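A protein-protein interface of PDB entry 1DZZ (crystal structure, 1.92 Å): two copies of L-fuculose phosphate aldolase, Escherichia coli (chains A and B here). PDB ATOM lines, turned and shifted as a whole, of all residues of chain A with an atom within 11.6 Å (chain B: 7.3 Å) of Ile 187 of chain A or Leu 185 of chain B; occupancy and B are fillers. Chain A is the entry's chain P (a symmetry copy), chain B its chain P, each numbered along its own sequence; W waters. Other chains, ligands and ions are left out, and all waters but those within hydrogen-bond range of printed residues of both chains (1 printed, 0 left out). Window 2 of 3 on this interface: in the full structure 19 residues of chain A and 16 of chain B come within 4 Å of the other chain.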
ATOM      1  N   LEU A 104      15.495 -11.521 -18.792  1.00  0.00           N
ATOM      2  CA  LEU A 104      16.436 -12.460 -18.173  1.00  0.00           C
ATOM      3  C   LEU A 104      16.174 -13.849 -18.750  1.00  0.00           C
ATOM      4  O   LEU A 104      16.926 -14.774 -18.463  1.00  0.00           O
ATOM      5  CB  LEU A 104      16.352 -12.486 -16.647  1.00  0.00           C
ATOM      6  CG  LEU A 104      16.529 -11.162 -15.898  1.00  0.00           C
ATOM      7  CD1 LEU A 104      16.358 -11.305 -14.391  1.00  0.00           C
ATOM      8  CD2 LEU A 104      17.881 -10.539 -16.173  1.00  0.00           C
ATOM      9  N   ARG A 106      13.836 -16.054 -17.984  1.00  0.00           N
ATOM     10  CA  ARG A 106      13.603 -16.990 -16.891  1.00  0.00           C
ATOM     11  C   ARG A 106      12.130 -17.325 -16.774  1.00  0.00           C
ATOM     12  O   ARG A 106      11.304 -16.425 -17.011  1.00  0.00           O
ATOM     13  CB  ARG A 106      14.000 -16.245 -15.595  1.00  0.00           C
ATOM     14  CG  ARG A 106      15.511 -16.113 -15.442  1.00  0.00           C
ATOM     15  CD  ARG A 106      15.778 -16.217 -13.933  1.00  0.00           C
ATOM     16  NE  ARG A 106      17.083 -15.665 -13.644  1.00  0.00           N
ATOM     17  CZ  ARG A 106      17.769 -15.898 -12.529  1.00  0.00           C
ATOM     18  NH1 ARG A 106      17.258 -16.685 -11.597  1.00  0.00           N
ATOM     19  NH2 ARG A 106      18.963 -15.320 -12.409  1.00  0.00           N
ATOM     20  N   ALA A 178       5.727 -11.589 -10.919  1.00  0.00           N
ATOM     21  CA  ALA A 178       6.972 -11.100 -11.519  1.00  0.00           C
ATOM     22  C   ALA A 178       7.711 -10.111 -10.617  1.00  0.00           C
ATOM     23  O   ALA A 178       8.917 -10.210 -10.397  1.00  0.00           O
ATOM     24  CB  ALA A 178       6.644 -10.464 -12.877  1.00  0.00           C
ATOM     25  N   GLN A 179       6.951  -9.185 -10.023  1.00  0.00           N
ATOM     26  CA  GLN A 179       7.467  -8.207  -9.099  1.00  0.00           C
ATOM     27  C   GLN A 179       8.012  -8.877  -7.840  1.00  0.00           C
ATOM     28  O   GLN A 179       9.140  -8.581  -7.459  1.00  0.00           O
ATOM     29  CB  GLN A 179       6.409  -7.151  -8.741  1.00  0.00           C
ATOM     30  CG  GLN A 179       7.093  -6.090  -7.873  1.00  0.00           C
ATOM     31  CD  GLN A 179       6.190  -4.920  -7.544  1.00  0.00           C
ATOM     32  OE1 GLN A 179       5.031  -4.908  -7.938  1.00  0.00           O
ATOM     33  NE2 GLN A 179       6.769  -3.963  -6.818  1.00  0.00           N
ATOM     34  N   LEU A 180       7.292  -9.855  -7.303  1.00  0.00           N
ATOM     35  CA  LEU A 180       7.762 -10.638  -6.172  1.00  0.00           C
ATOM     36  C   LEU A 180       9.086 -11.330  -6.490  1.00  0.00           C
ATOM     37  O   LEU A 180      10.032 -11.284  -5.705  1.00  0.00           O
ATOM     38  CB  LEU A 180       6.760 -11.732  -5.743  1.00  0.00           C
ATOM     39  CG  LEU A 180       5.497 -11.199  -5.057  1.00  0.00           C
ATOM     40  CD1 LEU A 180       4.528 -12.341  -4.848  1.00  0.00           C
ATOM     41  CD2 LEU A 180       5.843 -10.500  -3.729  1.00  0.00           C
ATOM     42  N   TYR A 181       9.183 -11.933  -7.663  1.00  0.00           N
ATOM     43  CA  TYR A 181      10.373 -12.636  -8.114  1.00  0.00           C
ATOM     44  C   TYR A 181      11.566 -11.712  -8.283  1.00  0.00           C
ATOM     45  O   TYR A 181      12.646 -12.021  -7.760  1.00  0.00           O
ATOM     46  CB  TYR A 181      10.047 -13.349  -9.448  1.00  0.00           C
ATOM     47  CG  TYR A 181      11.096 -14.369  -9.844  1.00  0.00           C
ATOM     48  CD1 TYR A 181      11.780 -15.089  -8.856  1.00  0.00           C
ATOM     49  CD2 TYR A 181      11.389 -14.615 -11.178  1.00  0.00           C
ATOM     50  CE1 TYR A 181      12.725 -16.016  -9.207  1.00  0.00           C
ATOM     51  CE2 TYR A 181      12.338 -15.550 -11.538  1.00  0.00           C
ATOM     52  CZ  TYR A 181      12.997 -16.242 -10.533  1.00  0.00           C
ATOM     53  OH  TYR A 181      13.955 -17.180 -10.848  1.00  0.00           O
ATOM     54  N   LEU A 182      11.386 -10.573  -8.946  1.00  0.00           N
ATOM     55  CA  LEU A 182      12.503  -9.659  -9.146  1.00  0.00           C
ATOM     56  C   LEU A 182      12.996  -9.027  -7.847  1.00  0.00           C
ATOM     57  O   LEU A 182      14.202  -8.814  -7.654  1.00  0.00           O
ATOM     58  CB  LEU A 182      12.139  -8.541 -10.116  1.00  0.00           C
ATOM     59  CG  LEU A 182      11.801  -8.913 -11.558  1.00  0.00           C
ATOM     60  CD1 LEU A 182      10.946  -7.804 -12.175  1.00  0.00           C
ATOM     61  CD2 LEU A 182      13.088  -9.119 -12.340  1.00  0.00           C
ATOM     62  N   THR A 183      12.068  -8.688  -6.949  1.00  0.00           N
ATOM     63  CA  THR A 183      12.423  -8.096  -5.662  1.00  0.00           C
ATOM     64  C   THR A 183      13.215  -9.077  -4.808  1.00  0.00           C
ATOM     65  O   THR A 183      14.235  -8.704  -4.232  1.00  0.00           O
ATOM     66  CB  THR A 183      11.124  -7.712  -4.921  1.00  0.00           C
ATOM     67  OG1 THR A 183      10.448  -6.801  -5.806  1.00  0.00           O
ATOM     68  CG2 THR A 183      11.414  -7.023  -3.602  1.00  0.00           C
ATOM     69  N   THR A 184      12.819 -10.342  -4.805  1.00  0.00           N
ATOM     70  CA  THR A 184      13.517 -11.348  -4.021  1.00  0.00           C
ATOM     71  C   THR A 184      14.807 -11.804  -4.707  1.00  0.00           C
ATOM     72  O   THR A 184      15.834 -11.950  -4.021  1.00  0.00           O
ATOM     73  CB  THR A 184      12.582 -12.525  -3.684  1.00  0.00           C
ATOM     74  OG1 THR A 184      11.986 -13.053  -4.881  1.00  0.00           O
ATOM     75  CG2 THR A 184      11.532 -12.012  -2.715  1.00  0.00           C
ATOM     76  N   LEU A 185      14.851 -11.864  -6.030  1.00  0.00           N
ATOM     77  CA  LEU A 185      16.030 -12.247  -6.779  1.00  0.00           C
ATOM     78  C   LEU A 185      17.198 -11.292  -6.561  1.00  0.00           C
ATOM     79  O   LEU A 185      18.349 -11.710  -6.606  1.00  0.00           O
ATOM     80  CB  LEU A 185      15.715 -12.264  -8.285  1.00  0.00           C
ATOM     81  CG  LEU A 185      16.368 -13.285  -9.184  1.00  0.00           C
ATOM     82  CD1 LEU A 185      16.442 -14.680  -8.608  1.00  0.00           C
ATOM     83  CD2 LEU A 185      15.664 -13.303 -10.549  1.00  0.00           C
ATOM     84  N   ALA A 186      16.920 -10.022  -6.317  1.00  0.00           N
ATOM     85  CA  ALA A 186      17.924  -9.011  -6.075  1.00  0.00           C
ATOM     86  C   ALA A 186      18.613  -9.206  -4.724  1.00  0.00           C
ATOM     87  O   ALA A 186      19.723  -8.719  -4.504  1.00  0.00           O
ATOM     88  CB  ALA A 186      17.275  -7.636  -6.190  1.00  0.00           C
ATOM     89  N   ILE A 187      17.977  -9.917  -3.820  1.00  0.00           N
ATOM     90  CA  ILE A 187      18.461 -10.251  -2.504  1.00  0.00           C
ATOM     91  C   ILE A 187      19.099 -11.643  -2.490  1.00  0.00           C
ATOM     92  O   ILE A 187      20.174 -11.739  -1.918  1.00  0.00           O
ATOM     93  CB  ILE A 187      17.333 -10.315  -1.455  1.00  0.00           C
ATOM     94  CG1 ILE A 187      16.531  -9.012  -1.455  1.00  0.00           C
ATOM     95  CG2 ILE A 187      17.848 -10.656  -0.062  1.00  0.00           C
ATOM     96  CD1 ILE A 187      17.317  -7.763  -1.272  1.00  0.00           C
ATOM     97  N   THR A 188      18.412 -12.667  -2.974  1.00  0.00           N
ATOM     98  CA  THR A 188      18.969 -14.007  -2.918  1.00  0.00           C
ATOM     99  C   THR A 188      18.676 -14.800  -4.187  1.00  0.00           C
ATOM    100  O   THR A 188      17.578 -14.689  -4.730  1.00  0.00           O
ATOM    101  CB  THR A 188      18.476 -14.767  -1.674  1.00  0.00           C
ATOM    102  OG1 THR A 188      19.157 -16.030  -1.678  1.00  0.00           O
ATOM    103  CG2 THR A 188      16.990 -15.070  -1.706  1.00  0.00           C
ATOM    104  N   ASP A 189      19.641 -15.557  -4.690  1.00  0.00           N
ATOM    105  CA  ASP A 189      19.524 -16.359  -5.907  1.00  0.00           C
ATOM    106  C   ASP A 189      20.133 -17.731  -5.646  1.00  0.00           C
ATOM    107  O   ASP A 189      21.331 -17.777  -5.333  1.00  0.00           O
ATOM    108  CB  ASP A 189      20.287 -15.687  -7.057  1.00  0.00           C
ATOM    109  CG  ASP A 189      19.989 -16.305  -8.408  1.00  0.00           C
ATOM    110  OD1 ASP A 189      19.355 -17.379  -8.486  1.00  0.00           O
ATOM    111  OD2 ASP A 189      20.369 -15.729  -9.448  1.00  0.00           O
ATOM    112  N   PRO A 190      19.325 -18.788  -5.675  1.00  0.00           N
ATOM    113  CA  PRO A 190      17.937 -18.758  -6.063  1.00  0.00           C
ATOM    114  C   PRO A 190      16.918 -18.387  -4.997  1.00  0.00           C
ATOM    115  O   PRO A 190      17.238 -18.321  -3.813  1.00  0.00           O
ATOM    116  CB  PRO A 190      17.675 -20.206  -6.533  1.00  0.00           C
ATOM    117  CG  PRO A 190      18.548 -21.034  -5.652  1.00  0.00           C
ATOM    118  CD  PRO A 190      19.774 -20.179  -5.411  1.00  0.00           C
ATOM    119  N   VAL A 191      15.681 -18.138  -5.419  1.00  0.00           N
ATOM    120  CA  VAL A 191      14.617 -17.755  -4.478  1.00  0.00           C
ATOM    121  C   VAL A 191      13.951 -19.012  -3.936  1.00  0.00           C
ATOM    122  O   VAL A 191      13.673 -19.940  -4.677  1.00  0.00           O
ATOM    123  CB  VAL A 191      13.544 -16.863  -5.156  1.00  0.00           C
ATOM    124  CG1 VAL A 191      12.438 -16.506  -4.150  1.00  0.00           C
ATOM    125  CG2 VAL A 191      14.113 -15.564  -5.708  1.00  0.00           C
ATOM    126  N   PRO A 192      13.653 -19.052  -2.644  1.00  0.00           N
ATOM    127  CA  PRO A 192      12.971 -20.194  -2.046  1.00  0.00           C
ATOM    128  C   PRO A 192      11.690 -20.460  -2.811  1.00  0.00           C
ATOM    129  O   PRO A 192      11.051 -19.492  -3.204  1.00  0.00           O
ATOM    130  CB  PRO A 192      12.666 -19.745  -0.613  1.00  0.00           C
ATOM    131  CG  PRO A 192      13.741 -18.741  -0.342  1.00  0.00           C
ATOM    132  CD  PRO A 192      13.974 -18.015  -1.653  1.00  0.00           C
ATOM    133  N   VAL B 101       8.994 -10.223   1.575  1.00  0.00           N
ATOM    134  CA  VAL B 101       9.744 -10.552   2.787  1.00  0.00           C
ATOM    135  C   VAL B 101       9.335 -11.943   3.283  1.00  0.00           C
ATOM    136  O   VAL B 101      10.196 -12.709   3.751  1.00  0.00           O
ATOM    137  CB  VAL B 101       9.565  -9.544   3.924  1.00  0.00           C
ATOM    138  CG1 VAL B 101      10.300  -9.990   5.202  1.00  0.00           C
ATOM    139  CG2 VAL B 101      10.070  -8.179   3.503  1.00  0.00           C
ATOM    140  N   LEU B 104      11.225 -14.765   1.611  1.00  0.00           N
ATOM    141  CA  LEU B 104      12.582 -14.952   2.135  1.00  0.00           C
ATOM    142  C   LEU B 104      12.477 -15.599   3.514  1.00  0.00           C
ATOM    143  O   LEU B 104      13.496 -15.960   4.091  1.00  0.00           O
ATOM    144  CB  LEU B 104      13.388 -13.656   2.208  1.00  0.00           C
ATOM    145  CG  LEU B 104      13.545 -12.837   0.925  1.00  0.00           C
ATOM    146  CD1 LEU B 104      14.310 -11.538   1.139  1.00  0.00           C
ATOM    147  CD2 LEU B 104      14.238 -13.629  -0.165  1.00  0.00           C
ATOM    148  N   ARG B 106      11.787 -14.239   6.445  1.00  0.00           N
ATOM    149  CA  ARG B 106      12.511 -13.424   7.412  1.00  0.00           C
ATOM    150  C   ARG B 106      11.550 -12.636   8.278  1.00  0.00           C
ATOM    151  O   ARG B 106      10.509 -12.201   7.751  1.00  0.00           O
ATOM    152  CB  ARG B 106      13.323 -12.398   6.588  1.00  0.00           C
ATOM    153  CG  ARG B 106      14.527 -13.028   5.900  1.00  0.00           C
ATOM    154  CD  ARG B 106      15.617 -11.946   5.913  1.00  0.00           C
ATOM    155  NE  ARG B 106      16.613 -12.265   4.915  1.00  0.00           N
ATOM    156  CZ  ARG B 106      17.840 -11.755   4.886  1.00  0.00           C
ATOM    157  NH1 ARG B 106      18.216 -10.895   5.818  1.00  0.00           N
ATOM    158  NH2 ARG B 106      18.649 -12.149   3.902  1.00  0.00           N
ATOM    159  N   GLN B 179       8.926  -2.568   2.762  1.00  0.00           N
ATOM    160  CA  GLN B 179       9.548  -1.858   1.672  1.00  0.00           C
ATOM    161  C   GLN B 179      10.881  -1.253   2.103  1.00  0.00           C
ATOM    162  O   GLN B 179      11.871  -1.460   1.409  1.00  0.00           O
ATOM    163  CB  GLN B 179       8.618  -0.778   1.096  1.00  0.00           C
ATOM    164  CG  GLN B 179       9.311  -0.184  -0.135  1.00  0.00           C
ATOM    165  CD  GLN B 179       8.449   0.817  -0.875  1.00  0.00           C
ATOM    166  OE1 GLN B 179       7.334   1.098  -0.456  1.00  0.00           O
ATOM    167  NE2 GLN B 179       9.014   1.326  -1.971  1.00  0.00           N
ATOM    168  N   LEU B 180      10.930  -0.652   3.286  1.00  0.00           N
ATOM    169  CA  LEU B 180      12.168  -0.138   3.848  1.00  0.00           C
ATOM    170  C   LEU B 180      13.213  -1.242   3.988  1.00  0.00           C
ATOM    171  O   LEU B 180      14.368  -1.078   3.599  1.00  0.00           O
ATOM    172  CB  LEU B 180      11.975   0.495   5.244  1.00  0.00           C
ATOM    173  CG  LEU B 180      11.232   1.837   5.232  1.00  0.00           C
ATOM    174  CD1 LEU B 180      10.955   2.261   6.657  1.00  0.00           C
ATOM    175  CD2 LEU B 180      12.036   2.906   4.471  1.00  0.00           C
ATOM    176  N   TYR B 181      12.807  -2.394   4.497  1.00  0.00           N
ATOM    177  CA  TYR B 181      13.678  -3.541   4.695  1.00  0.00           C
ATOM    178  C   TYR B 181      14.216  -4.096   3.389  1.00  0.00           C
ATOM    179  O   TYR B 181      15.434  -4.296   3.275  1.00  0.00           O
ATOM    180  CB  TYR B 181      12.890  -4.629   5.463  1.00  0.00           C
ATOM    181  CG  TYR B 181      13.780  -5.728   6.009  1.00  0.00           C
ATOM    182  CD1 TYR B 181      15.082  -5.429   6.431  1.00  0.00           C
ATOM    183  CD2 TYR B 181      13.325  -7.035   6.111  1.00  0.00           C
ATOM    184  CE1 TYR B 181      15.889  -6.416   6.931  1.00  0.00           C
ATOM    185  CE2 TYR B 181      14.132  -8.033   6.617  1.00  0.00           C
ATOM    186  CZ  TYR B 181      15.417  -7.701   7.021  1.00  0.00           C
ATOM    187  OH  TYR B 181      16.258  -8.667   7.527  1.00  0.00           O
ATOM    188  N   LEU B 182      13.356  -4.297   2.393  1.00  0.00           N
ATOM    189  CA  LEU B 182      13.822  -4.841   1.124  1.00  0.00           C
ATOM    190  C   LEU B 182      14.743  -3.887   0.369  1.00  0.00           C
ATOM    191  O   LEU B 182      15.712  -4.308  -0.280  1.00  0.00           O
ATOM    192  CB  LEU B 182      12.655  -5.203   0.213  1.00  0.00           C
ATOM    193  CG  LEU B 182      11.693  -6.299   0.668  1.00  0.00           C
ATOM    194  CD1 LEU B 182      10.351  -6.117  -0.045  1.00  0.00           C
ATOM    195  CD2 LEU B 182      12.300  -7.659   0.367  1.00  0.00           C
ATOM    196  N   THR B 183      14.436  -2.587   0.414  1.00  0.00           N
ATOM    197  CA  THR B 183      15.257  -1.580  -0.253  1.00  0.00           C
ATOM    198  C   THR B 183      16.645  -1.506   0.368  1.00  0.00           C
ATOM    199  O   THR B 183      17.640  -1.479  -0.354  1.00  0.00           O
ATOM    200  CB  THR B 183      14.564  -0.208  -0.112  1.00  0.00           C
ATOM    201  OG1 THR B 183      13.268  -0.384  -0.712  1.00  0.00           O
ATOM    202  CG2 THR B 183      15.323   0.881  -0.844  1.00  0.00           C
ATOM    203  N   THR B 184      16.728  -1.578   1.689  1.00  0.00           N
ATOM    204  CA  THR B 184      18.012  -1.518   2.368  1.00  0.00           C
ATOM    205  C   THR B 184      18.751  -2.855   2.298  1.00  0.00           C
ATOM    206  O   THR B 184      19.971  -2.857   2.054  1.00  0.00           O
ATOM    207  CB  THR B 184      17.844  -1.013   3.814  1.00  0.00           C
ATOM    208  OG1 THR B 184      16.870  -1.808   4.513  1.00  0.00           O
ATOM    209  CG2 THR B 184      17.431   0.446   3.745  1.00  0.00           C
ATOM    210  N   LEU B 185      18.055  -3.982   2.321  1.00  0.00           N
ATOM    211  CA  LEU B 185      18.651  -5.298   2.224  1.00  0.00           C
ATOM    212  C   LEU B 185      19.380  -5.515   0.903  1.00  0.00           C
ATOM    213  O   LEU B 185      20.363  -6.244   0.857  1.00  0.00           O
ATOM    214  CB  LEU B 185      17.563  -6.380   2.340  1.00  0.00           C
ATOM    215  CG  LEU B 185      17.865  -7.688   3.031  1.00  0.00           C
ATOM    216  CD1 LEU B 185      18.672  -7.560   4.302  1.00  0.00           C
ATOM    217  CD2 LEU B 185      16.560  -8.451   3.296  1.00  0.00           C
ATOM    218  N   ALA B 186      18.919  -4.888  -0.167  1.00  0.00           N
ATOM    219  CA  ALA B 186      19.518  -4.987  -1.478  1.00  0.00           C
ATOM    220  C   ALA B 186      20.870  -4.275  -1.541  1.00  0.00           C
ATOM    221  O   ALA B 186      21.697  -4.563  -2.407  1.00  0.00           O
ATOM    222  CB  ALA B 186      18.538  -4.439  -2.510  1.00  0.00           C
ATOM    223  N   ILE B 187      21.110  -3.356  -0.632  1.00  0.00           N
ATOM    224  CA  ILE B 187      22.327  -2.597  -0.489  1.00  0.00           C
ATOM    225  C   ILE B 187      23.247  -3.227   0.562  1.00  0.00           C
ATOM    226  O   ILE B 187      24.423  -3.336   0.253  1.00  0.00           O
ATOM    227  CB  ILE B 187      22.076  -1.159   0.007  1.00  0.00           C
ATOM    228  CG1 ILE B 187      21.064  -0.453  -0.899  1.00  0.00           C
ATOM    229  CG2 ILE B 187      23.362  -0.354   0.145  1.00  0.00           C
ATOM    230  CD1 ILE B 187      21.391  -0.434  -2.350  1.00  0.00           C
ATOM    231  N   THR B 188      22.757  -3.495   1.762  1.00  0.00           N
ATOM    232  CA  THR B 188      23.624  -4.036   2.796  1.00  0.00           C
ATOM    233  C   THR B 188      22.922  -5.105   3.626  1.00  0.00           C
ATOM    234  O   THR B 188      21.739  -4.957   3.929  1.00  0.00           O
ATOM    235  CB  THR B 188      24.180  -2.922   3.700  1.00  0.00           C
ATOM    236  OG1 THR B 188      25.083  -3.560   4.614  1.00  0.00           O
ATOM    237  CG2 THR B 188      23.115  -2.242   4.538  1.00  0.00           C
ATOM    238  N   ASP B 189      23.607  -6.191   3.958  1.00  0.00           N
ATOM    239  CA  ASP B 189      23.072  -7.310   4.731  1.00  0.00           C
ATOM    240  C   ASP B 189      24.103  -7.716   5.776  1.00  0.00           C
ATOM    241  O   ASP B 189      25.213  -8.093   5.372  1.00  0.00           O
ATOM    242  CB  ASP B 189      22.802  -8.507   3.808  1.00  0.00           C
ATOM    243  CG  ASP B 189      21.998  -9.603   4.477  1.00  0.00           C
ATOM    244  OD1 ASP B 189      21.794  -9.575   5.710  1.00  0.00           O
ATOM    245  OD2 ASP B 189      21.525 -10.530   3.788  1.00  0.00           O
ATOM    246  N   PRO B 190      23.789  -7.553   7.059  1.00  0.00           N
ATOM    247  CA  PRO B 190      22.496  -7.145   7.549  1.00  0.00           C
ATOM    248  C   PRO B 190      22.206  -5.653   7.600  1.00  0.00           C
ATOM    249  O   PRO B 190      23.100  -4.829   7.433  1.00  0.00           O
ATOM    250  CB  PRO B 190      22.470  -7.716   8.983  1.00  0.00           C
ATOM    251  CG  PRO B 190      23.889  -7.628   9.433  1.00  0.00           C
ATOM    252  CD  PRO B 190      24.705  -7.878   8.183  1.00  0.00           C
ATOM    253  N   VAL B 191      20.943  -5.302   7.830  1.00  0.00           N
ATOM    254  CA  VAL B 191      20.544  -3.887   7.886  1.00  0.00           C
ATOM    255  C   VAL B 191      20.721  -3.372   9.308  1.00  0.00           C
ATOM    256  O   VAL B 191      20.371  -4.043  10.263  1.00  0.00           O
ATOM    257  CB  VAL B 191      19.066  -3.690   7.455  1.00  0.00           C
ATOM    258  CG1 VAL B 191      18.679  -2.205   7.551  1.00  0.00           C
ATOM    259  CG2 VAL B 191      18.796  -4.153   6.031  1.00  0.00           C
HETATM  260  O   HOH W   1      22.038  -7.905  -3.134  1.00  0.00           O
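OG1 of Thr 183 of chain A is in hydrogen-bond range of O of Gln 179 of chain A.
Ile 187 of chain A touches Leu 104 of chain B, but with the chains exchanged Leu 104 of chain A does not touch Ile 187 of chain B (16.6 Å). Ile 187 of chain A touches Leu 182 of chain B, but with the chains exchanged Leu 182 of chain A does not touch Ile 187 of chain B (11.3 Å). Ile 187 of chain A touches Leu 185 of chain B, but with the chains exchanged Leu 185 of chain A does not touch Ile 187 of chain B (10.6 Å). Thr 188 of chain A touches Leu 104 of chain B, but with the chains exchanged Leu 104 of chain A does not touch Thr 188 of chain B (19.0 Å). 15 positions are printed for both chains.
Hydrophobic or aromatic side chains of chain B within 4 Å of the printed part of chain A: Leu 104, Leu 182, Leu 185 and Ala 186. Of the 17 printed residues of chain A, 3 touch a printed residue of chain B. Printed residues of chain A that touch a printed residue of chain B: Thr 183, Ile 187 and Thr 188. Hydrophobic or aromatic side chains of chain A that line the printed part of chain B: Ile 187.
Among the printed residues, pairs that only touch across the chains: Thr 183 of chain A with Leu 182 of chain B, Ile 187 of chain A with Leu 104 of chain B, Ile 187 of chain A with Leu 182 of chain B, Ile 187 of chain A with Leu 185 of chain B, Ile 187 of chain A with Ala 186 of chain B and Thr 188 of chain A with Leu 104 of chain B.
Of the printed residues of chain B, Thr 183 of chain A touches Leu 182 (3.8 Å). Ala 186 of chain A touches none of the printed residues of chain B. Of the printed residues of chain B, Thr 188 of chain A touches Leu 104 (3.5 Å). Pro 190 of chain A touches none of the printed residues of chain B. Of the printed residues of chain A, Leu 104 of chain B touches Ile 187 and Thr 188. No residue of chain A comes within 4 Å of Tyr 181 of chain B. Of chain A, only Thr 183 (3.8 Å) and Ile 187 (3.9 Å) come within 4 Å of Leu 182 of chain B. No residue of chain A comes within 4 Å of Thr 183 of chain B. Leu 185 of chain B touches just one residue of chain A: Ile 187 (3.7 Å). No residue of chain A comes within 4 Å of Ile 187 of chain B. Thr 188 of chain B touches none of the printed residues of chain A. No residue of chain A comes within 4 Å of Asp 189 of chain B. No residue of chain A comes within 4 Å of Pro 190 of chain B. No residue of chain A comes within 4 Å of Val 191 of chain B. The nearest residue of chain B that does not touch Ile 187 of chain A is Arg 106 of chain B (4.3 Å).
Water W1 bridges the backbone carbonyl oxygen (O) of Ala 186 of chain A (2.8 Å) and the backbone carbonyl oxygen (O) of Ala 186 of chain B (3.4 Å).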
